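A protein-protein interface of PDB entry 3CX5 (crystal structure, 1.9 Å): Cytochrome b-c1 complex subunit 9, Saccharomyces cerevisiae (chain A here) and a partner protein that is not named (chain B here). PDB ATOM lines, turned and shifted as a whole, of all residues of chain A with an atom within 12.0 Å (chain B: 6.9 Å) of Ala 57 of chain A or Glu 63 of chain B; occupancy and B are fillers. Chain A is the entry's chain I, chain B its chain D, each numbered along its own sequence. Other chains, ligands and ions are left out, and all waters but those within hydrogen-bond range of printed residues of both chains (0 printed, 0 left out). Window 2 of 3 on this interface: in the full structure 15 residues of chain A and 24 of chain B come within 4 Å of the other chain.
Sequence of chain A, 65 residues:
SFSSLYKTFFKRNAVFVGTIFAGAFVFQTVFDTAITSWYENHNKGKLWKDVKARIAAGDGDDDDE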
ATOM      1  N   TRP A  48      18.913  16.225   5.635  1.00  0.00           N
ATOM      2  CA  TRP A  48      19.114  17.660   5.471  1.00  0.00           C
ATOM      3  C   TRP A  48      18.983  18.080   4.005  1.00  0.00           C
ATOM      4  O   TRP A  48      18.442  19.143   3.715  1.00  0.00           O
ATOM      5  CB  TRP A  48      20.486  18.084   6.014  1.00  0.00           C
ATOM      6  CG  TRP A  48      20.861  19.505   5.660  1.00  0.00           C
ATOM      7  CD1 TRP A  48      21.927  19.906   4.905  1.00  0.00           C
ATOM      8  CD2 TRP A  48      20.158  20.700   6.023  1.00  0.00           C
ATOM      9  NE1 TRP A  48      21.932  21.273   4.777  1.00  0.00           N
ATOM     10  CE2 TRP A  48      20.857  21.786   5.452  1.00  0.00           C
ATOM     11  CE3 TRP A  48      19.001  20.959   6.770  1.00  0.00           C
ATOM     12  CZ2 TRP A  48      20.438  23.116   5.605  1.00  0.00           C
ATOM     13  CZ3 TRP A  48      18.582  22.283   6.923  1.00  0.00           C
ATOM     14  CH2 TRP A  48      19.304  23.342   6.341  1.00  0.00           C
ATOM     15  N   LYS A  49      19.477  17.246   3.092  1.00  0.00           N
ATOM     16  CA  LYS A  49      19.403  17.539   1.656  1.00  0.00           C
ATOM     17  C   LYS A  49      17.949  17.744   1.258  1.00  0.00           C
ATOM     18  O   LYS A  49      17.619  18.663   0.508  1.00  0.00           O
ATOM     19  CB  LYS A  49      19.937  16.377   0.820  1.00  0.00           C
ATOM     20  CG  LYS A  49      21.328  15.894   1.146  1.00  0.00           C
ATOM     21  CD  LYS A  49      21.731  14.794   0.164  1.00  0.00           C
ATOM     22  CE  LYS A  49      20.658  13.710   0.072  1.00  0.00           C
ATOM     23  NZ  LYS A  49      21.005  12.652  -0.918  1.00  0.00           N
ATOM     24  N   VAL A  51      15.437  18.448   3.329  1.00  0.00           N
ATOM     25  CA  VAL A  51      14.892  19.595   4.049  1.00  0.00           C
ATOM     26  C   VAL A  51      15.339  20.906   3.412  1.00  0.00           C
ATOM     27  O   VAL A  51      14.554  21.847   3.299  1.00  0.00           O
ATOM     28  CB  VAL A  51      15.307  19.580   5.543  1.00  0.00           C
ATOM     29  CG1 VAL A  51      14.717  20.781   6.272  1.00  0.00           C
ATOM     30  CG2 VAL A  51      14.847  18.290   6.205  1.00  0.00           C
ATOM     31  N   LYS A  52      16.599  20.953   2.988  1.00  0.00           N
ATOM     32  CA  LYS A  52      17.166  22.141   2.355  1.00  0.00           C
ATOM     33  C   LYS A  52      16.466  22.439   1.027  1.00  0.00           C
ATOM     34  O   LYS A  52      16.364  23.596   0.618  1.00  0.00           O
ATOM     35  CB  LYS A  52      18.670  21.951   2.127  1.00  0.00           C
ATOM     36  CG  LYS A  52      19.396  23.202   1.668  1.00  0.00           C
ATOM     37  CD  LYS A  52      20.871  22.938   1.411  1.00  0.00           C
ATOM     38  CE  LYS A  52      21.568  24.183   0.882  1.00  0.00           C
ATOM     39  NZ  LYS A  52      23.007  23.941   0.584  1.00  0.00           N
ATOM     40  N   ALA A  53      15.977  21.390   0.368  1.00  0.00           N
ATOM     41  CA  ALA A  53      15.280  21.528  -0.909  1.00  0.00           C
ATOM     42  C   ALA A  53      14.076  22.465  -0.784  1.00  0.00           C
ATOM     43  O   ALA A  53      13.872  23.340  -1.627  1.00  0.00           O
ATOM     44  CB  ALA A  53      14.839  20.160  -1.421  1.00  0.00           C
ATOM     45  N   ARG A  54      13.297  22.290   0.281  1.00  0.00           N
ATOM     46  CA  ARG A  54      12.122  23.123   0.524  1.00  0.00           C
ATOM     47  C   ARG A  54      12.509  24.394   1.280  1.00  0.00           C
ATOM     48  O   ARG A  54      12.335  25.507   0.779  1.00  0.00           O
ATOM     49  CB  ARG A  54      11.083  22.352   1.343  1.00  0.00           C
ATOM     50  CG  ARG A  54      10.734  20.969   0.807  1.00  0.00           C
ATOM     51  CD  ARG A  54      11.165  19.875   1.781  1.00  0.00           C
ATOM     52  NE  ARG A  54      10.650  20.106   3.131  1.00  0.00           N
ATOM     53  CZ  ARG A  54      10.801  19.266   4.154  1.00  0.00           C
ATOM     54  NH1 ARG A  54      11.454  18.120   3.993  1.00  0.00           N
ATOM     55  NH2 ARG A  54      10.314  19.582   5.347  1.00  0.00           N
ATOM     56  N   ILE A  55      13.047  24.206   2.483  1.00  0.00           N
ATOM     57  CA  ILE A  55      13.469  25.299   3.360  1.00  0.00           C
ATOM     58  C   ILE A  55      14.587  26.154   2.759  1.00  0.00           C
ATOM     59  O   ILE A  55      15.481  25.642   2.081  1.00  0.00           O
ATOM     60  CB  ILE A  55      13.929  24.746   4.741  1.00  0.00           C
ATOM     61  CG1 ILE A  55      12.787  23.976   5.415  1.00  0.00           C
ATOM     62  CG2 ILE A  55      14.422  25.872   5.642  1.00  0.00           C
ATOM     63  CD1 ILE A  55      11.533  24.798   5.668  1.00  0.00           C
ATOM     64  N   ALA A  56      14.522  27.459   3.020  1.00  0.00           N
ATOM     65  CA  ALA A  56      15.512  28.421   2.531  1.00  0.00           C
ATOM     66  C   ALA A  56      15.426  29.738   3.313  1.00  0.00           C
ATOM     67  O   ALA A  56      14.577  29.895   4.196  1.00  0.00           O
ATOM     68  CB  ALA A  56      15.311  28.676   1.033  1.00  0.00           C
ATOM     69  N   ALA A  57      16.315  30.675   2.989  1.00  0.00           N
ATOM     70  CA  ALA A  57      16.350  31.980   3.649  1.00  0.00           C
ATOM     71  C   ALA A  57      17.057  33.021   2.781  1.00  0.00           C
ATOM     72  O   ALA A  57      18.216  32.772   2.375  1.00  0.00           O
ATOM     73  CB  ALA A  57      17.037  31.867   5.012  1.00  0.00           C
ATOM     74  N   ARG B  30      16.054  21.293  13.234  1.00  0.00           N
ATOM     75  CA  ARG B  30      16.044  22.717  12.901  1.00  0.00           C
ATOM     76  C   ARG B  30      15.051  23.510  13.741  1.00  0.00           C
ATOM     77  O   ARG B  30      15.401  24.551  14.294  1.00  0.00           O
ATOM     78  CB  ARG B  30      15.750  22.915  11.412  1.00  0.00           C
ATOM     79  CG  ARG B  30      15.733  24.370  10.972  1.00  0.00           C
ATOM     80  CD  ARG B  30      15.632  24.473   9.460  1.00  0.00           C
ATOM     81  NE  ARG B  30      15.499  25.857   9.020  1.00  0.00           N
ATOM     82  CZ  ARG B  30      16.492  26.611   8.561  1.00  0.00           C
ATOM     83  NH1 ARG B  30      16.246  27.864   8.190  1.00  0.00           N
ATOM     84  NH2 ARG B  30      17.725  26.120   8.454  1.00  0.00           N
ATOM     85  N   TRP B  51      29.483  25.830  16.747  1.00  0.00           N
ATOM     86  CA  TRP B  51      28.642  26.385  15.689  1.00  0.00           C
ATOM     87  C   TRP B  51      28.744  25.598  14.389  1.00  0.00           C
ATOM     88  O   TRP B  51      27.723  25.258  13.784  1.00  0.00           O
ATOM     89  CB  TRP B  51      28.992  27.855  15.435  1.00  0.00           C
ATOM     90  CG  TRP B  51      28.546  28.790  16.521  1.00  0.00           C
ATOM     91  CD1 TRP B  51      29.343  29.497  17.368  1.00  0.00           C
ATOM     92  CD2 TRP B  51      27.197  29.147  16.851  1.00  0.00           C
ATOM     93  NE1 TRP B  51      28.583  30.276  18.199  1.00  0.00           N
ATOM     94  CE2 TRP B  51      27.260  30.084  17.903  1.00  0.00           C
ATOM     95  CE3 TRP B  51      25.940  28.769  16.356  1.00  0.00           C
ATOM     96  CZ2 TRP B  51      26.114  30.654  18.473  1.00  0.00           C
ATOM     97  CZ3 TRP B  51      24.800  29.333  16.924  1.00  0.00           C
ATOM     98  CH2 TRP B  51      24.898  30.267  17.972  1.00  0.00           C
ATOM     99  N   SER B  58      21.273  21.165  10.275  1.00  0.00           N
ATOM    100  CA  SER B  58      20.032  21.876  10.529  1.00  0.00           C
ATOM    101  C   SER B  58      20.003  23.254   9.872  1.00  0.00           C
ATOM    102  O   SER B  58      18.936  23.862   9.756  1.00  0.00           O
ATOM    103  CB  SER B  58      19.827  22.026  12.037  1.00  0.00           C
ATOM    104  OG  SER B  58      20.924  22.704  12.621  1.00  0.00           O
ATOM    105  N   HIS B  59      21.170  23.735   9.442  1.00  0.00           N
ATOM    106  CA  HIS B  59      21.300  25.051   8.811  1.00  0.00           C
ATOM    107  C   HIS B  59      22.408  25.084   7.766  1.00  0.00           C
ATOM    108  O   HIS B  59      23.208  24.152   7.658  1.00  0.00           O
ATOM    109  CB  HIS B  59      21.637  26.114   9.854  1.00  0.00           C
ATOM    110  CG  HIS B  59      20.627  26.238  10.948  1.00  0.00           C
ATOM    111  ND1 HIS B  59      20.613  25.403  12.044  1.00  0.00           N
ATOM    112  CD2 HIS B  59      19.619  27.123  11.133  1.00  0.00           C
ATOM    113  CE1 HIS B  59      19.641  25.768  12.860  1.00  0.00           C
ATOM    114  NE2 HIS B  59      19.023  26.809  12.331  1.00  0.00           N
ATOM    115  N   THR B  60      22.454  26.177   7.006  1.00  0.00           N
ATOM    116  CA  THR B  60      23.483  26.372   5.987  1.00  0.00           C
ATOM    117  C   THR B  60      24.668  27.084   6.637  1.00  0.00           C
ATOM    118  O   THR B  60      24.548  27.639   7.733  1.00  0.00           O
ATOM    119  CB  THR B  60      22.994  27.267   4.826  1.00  0.00           C
ATOM    120  OG1 THR B  60      22.650  28.559   5.341  1.00  0.00           O
ATOM    121  CG2 THR B  60      21.782  26.652   4.133  1.00  0.00           C
ATOM    122  N   ASN B  61      25.798  27.087   5.943  1.00  0.00           N
ATOM    123  CA  ASN B  61      27.003  27.739   6.431  1.00  0.00           C
ATOM    124  C   ASN B  61      26.710  29.216   6.685  1.00  0.00           C
ATOM    125  O   ASN B  61      27.060  29.768   7.734  1.00  0.00           O
ATOM    126  CB  ASN B  61      28.123  27.576   5.397  1.00  0.00           C
ATOM    127  CG  ASN B  61      29.423  28.224   5.832  1.00  0.00           C
ATOM    128  OD1 ASN B  61      29.593  29.433   5.697  1.00  0.00           O
ATOM    129  ND2 ASN B  61      30.349  27.420   6.357  1.00  0.00           N
ATOM    130  N   GLU B  62      26.001  29.826   5.740  1.00  0.00           N
ATOM    131  CA  GLU B  62      25.632  31.232   5.811  1.00  0.00           C
ATOM    132  C   GLU B  62      24.779  31.532   7.043  1.00  0.00           C
ATOM    133  O   GLU B  62      25.058  32.475   7.782  1.00  0.00           O
ATOM    134  CB  GLU B  62      24.882  31.640   4.537  1.00  0.00           C
ATOM    135  CG  GLU B  62      25.671  31.460   3.231  1.00  0.00           C
ATOM    136  CD  GLU B  62      26.043  30.003   2.923  1.00  0.00           C
ATOM    137  OE1 GLU B  62      25.160  29.118   2.986  1.00  0.00           O
ATOM    138  OE2 GLU B  62      27.230  29.745   2.614  1.00  0.00           O
ATOM    139  N   GLU B  63      23.749  30.720   7.266  1.00  0.00           N
ATOM    140  CA  GLU B  63      22.864  30.899   8.411  1.00  0.00           C
ATOM    141  C   GLU B  63      23.604  30.766   9.737  1.00  0.00           C
ATOM    142  O   GLU B  63      23.390  31.567  10.646  1.00  0.00           O
ATOM    143  CB  GLU B  63      21.710  29.897   8.363  1.00  0.00           C
ATOM    144  CG  GLU B  63      20.754  30.096   7.193  1.00  0.00           C
ATOM    145  CD  GLU B  63      19.673  29.029   7.132  1.00  0.00           C
ATOM    146  OE1 GLU B  63      18.506  29.379   6.864  1.00  0.00           O
ATOM    147  OE2 GLU B  63      19.985  27.840   7.351  1.00  0.00           O
ATOM    148  N   VAL B  64      24.481  29.769   9.842  1.00  0.00           N
ATOM    149  CA  VAL B  64      25.242  29.557  11.075  1.00  0.00           C
ATOM    150  C   VAL B  64      26.231  30.697  11.321  1.00  0.00           C
ATOM    151  O   VAL B  64      26.392  31.152  12.453  1.00  0.00           O
ATOM    152  CB  VAL B  64      25.974  28.186  11.075  1.00  0.00           C
ATOM    153  CG1 VAL B  64      26.772  28.013  12.361  1.00  0.00           C
ATOM    154  CG2 VAL B  64      24.959  27.053  10.949  1.00  0.00           C
ATOM    155  N   ARG B  65      26.865  31.181  10.255  1.00  0.00           N
ATOM    156  CA  ARG B  65      27.810  32.287  10.385  1.00  0.00           C
ATOM    157  C   ARG B  65      27.094  33.524  10.933  1.00  0.00           C
ATOM    158  O   ARG B  65      27.609  34.201  11.826  1.00  0.00           O
ATOM    159  CB  ARG B  65      28.484  32.605   9.046  1.00  0.00           C
ATOM    160  CG  ARG B  65      29.466  33.769   9.128  1.00  0.00           C
ATOM    161  CD  ARG B  65      30.177  34.030   7.808  1.00  0.00           C
ATOM    162  NE  ARG B  65      31.025  32.905   7.429  1.00  0.00           N
ATOM    163  CZ  ARG B  65      30.780  32.093   6.406  1.00  0.00           C
ATOM    164  NH1 ARG B  65      31.612  31.091   6.147  1.00  0.00           N
ATOM    165  NH2 ARG B  65      29.714  32.287   5.635  1.00  0.00           N
ATOM    166  N   ASN B  66      25.888  33.786  10.426  1.00  0.00           N
ATOM    167  CA  ASN B  66      25.097  34.926  10.885  1.00  0.00           C
ATOM    168  C   ASN B  66      24.682  34.737  12.342  1.00  0.00           C
ATOM    169  O   ASN B  66      24.636  35.697  13.101  1.00  0.00           O
ATOM    170  CB  ASN B  66      23.852  35.129  10.013  1.00  0.00           C
ATOM    171  CG  ASN B  66      24.190  35.526   8.577  1.00  0.00           C
ATOM    172  OD1 ASN B  66      23.423  35.251   7.651  1.00  0.00           O
ATOM    173  ND2 ASN B  66      25.337  36.170   8.388  1.00  0.00           N
ATOM    174  N   MET B  67      24.387  33.498  12.732  1.00  0.00           N
ATOM    175  CA  MET B  67      23.992  33.215  14.112  1.00  0.00           C
ATOM    176  C   MET B  67      25.158  33.395  15.075  1.00  0.00           C
ATOM    177  O   MET B  67      24.999  33.953  16.161  1.00  0.00           O
ATOM    178  CB  MET B  67      23.447  31.795  14.247  1.00  0.00           C
ATOM    179  CG  MET B  67      22.104  31.562  13.591  1.00  0.00           C
ATOM    180  SD  MET B  67      21.462  29.952  14.061  1.00  0.00           S
ATOM    181  CE  MET B  67      22.136  28.940  12.788  1.00  0.00           C
ATOM    182  N   ALA B  68      26.330  32.920  14.665  1.00  0.00           N
ATOM    183  CA  ALA B  68      27.530  33.016  15.491  1.00  0.00           C
ATOM    184  C   ALA B  68      27.934  34.473  15.733  1.00  0.00           C
ATOM    185  O   ALA B  68      28.254  34.862  16.858  1.00  0.00           O
ATOM    186  CB  ALA B  68      28.684  32.237  14.838  1.00  0.00           C
ATOM    187  N   GLU B  70      26.196  37.027  16.057  1.00  0.00           N
ATOM    188  CA  GLU B  70      25.292  37.780  16.922  1.00  0.00           C
ATOM    189  C   GLU B  70      25.823  37.800  18.358  1.00  0.00           C
ATOM    190  O   GLU B  70      25.350  38.570  19.193  1.00  0.00           O
ATOM    191  CB  GLU B  70      23.877  37.196  16.880  1.00  0.00           C
ATOM    192  CG  GLU B  70      23.193  37.354  15.528  1.00  0.00           C
ATOM    193  CD  GLU B  70      21.739  36.912  15.541  1.00  0.00           C
ATOM    194  OE1 GLU B  70      20.857  37.782  15.719  1.00  0.00           O
ATOM    195  OE2 GLU B  70      21.478  35.700  15.367  1.00  0.00           O
ATOM    196  N   LEU B  90      32.466  30.216  13.171  1.00  0.00           N
ATOM    197  CA  LEU B  90      32.097  28.804  13.103  1.00  0.00           C
ATOM    198  C   LEU B  90      32.843  27.890  14.073  1.00  0.00           C
ATOM    199  O   LEU B  90      32.285  26.895  14.525  1.00  0.00           O
ATOM    200  CB  LEU B  90      32.237  28.263  11.672  1.00  0.00           C
ATOM    201  CG  LEU B  90      31.378  28.886  10.563  1.00  0.00           C
ATOM    202  CD1 LEU B  90      31.603  28.129   9.269  1.00  0.00           C
ATOM    203  CD2 LEU B  90      29.907  28.858  10.925  1.00  0.00           C
ATOM    204  N   GLU B 176       9.353  29.094  11.435  1.00  0.00           N
ATOM    205  CA  GLU B 176       9.643  29.614  10.105  1.00  0.00           C
ATOM    206  C   GLU B 176       8.889  28.870   9.000  1.00  0.00           C
ATOM    207  O   GLU B 176       8.377  29.494   8.067  1.00  0.00           O
ATOM    208  CB  GLU B 176      11.152  29.533   9.857  1.00  0.00           C
ATOM    209  CG  GLU B 176      11.633  30.150   8.548  1.00  0.00           C
ATOM    210  CD  GLU B 176      13.142  30.034   8.354  1.00  0.00           C
ATOM    211  OE1 GLU B 176      13.616  30.315   7.230  1.00  0.00           O
ATOM    212  OE2 GLU B 176      13.856  29.665   9.316  1.00  0.00           O
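The backbone carbonyl oxygen (O) of Ala 56 of chain A lies close to the side-chain carboxylate (OE1) of Glu 176 of chain B, 3.2 Å away.
N of Thr 60 of chain B is in hydrogen-bond range of OE2 of Glu 63 of chain B, 3.0 Å away. The guanidinium group (NH1) of Arg 30 of chain B lies within salt-bridge range of the side-chain carboxylate (OE1) of Glu 63 of chain B, at 3.0 Å. OE2 of Glu 176 of chain B is in salt-bridge range of NH1 of Arg 30 of chain B (3.2 Å). The guanidinium group (NH2) of Arg 30 of chain B is in hydrogen-bond range of the backbone carbonyl oxygen (O) of Ser 58 of chain B, 2.9 Å away. The side-chain hydroxyl (OG) of Ser 58 of chain B lies within hydrogen-bond range of a ring nitrogen (ND1) of His 59 of chain B, at 2.8 Å. OE1 of Glu 62 of chain B sits close to OG1 of Thr 60 of chain B, at 3.5 Å.
Among the printed residues, merely in contact across the chains: Trp 48 of chain A with Arg 30 of chain B (3.8 Å), Trp 48 of chain A with Ser 58 of chain B (3.3 Å), Trp 48 of chain A with His 59 of chain B (3.5 Å), Trp 48 of chain A with Thr 60 of chain B (3.9 Å), Ile 55 of chain A with Arg 30 of chain B (3.5 Å) and Ala 57 of chain A with Glu 63 of chain B (3.4 Å).
Of chain A, only Ala 57 comes within 4 Å of Glu 63 of chain B. Ser 58 of chain B touches just one residue of chain A: Trp 48 (3.3 Å). Of chain A, only Trp 48 comes within 4 Å of His 59 of chain B. Thr 60 of chain B touches just one residue of chain A: Trp 48. No residue of chain A comes within 4 Å of Asn 61 of chain B. No residue of chain A comes within 4 Å of Glu 62 of chain B. No residue of chain A comes within 4 Å of Val 64 of chain B. No residue of chain A comes within 4 Å of Asn 66 of chain B. No residue of chain A comes within 4 Å of Met 67 of chain B. Of the printed residues of chain B, Ala 56 of chain A touches Glu 176. Of the printed residues of chain A, Arg 30 of chain B touches Trp 48 (3.8 Å) and Ile 55 (3.5 Å). Of the printed residues of chain A, Glu 176 of chain B touches Ala 56 (3.2 Å). Of the printed residues of chain B, Ile 55 of chain A touches Arg 30 (3.5 Å). Glu 70 of chain B touches none of the printed residues of chain A.
Printed residues of chain B that touch a printed residue of chain A: Arg 30, Ser 58, His 59, Thr 60, Glu 63 and Glu 176. Among the printed residues, 7 pairs touch across the chains.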
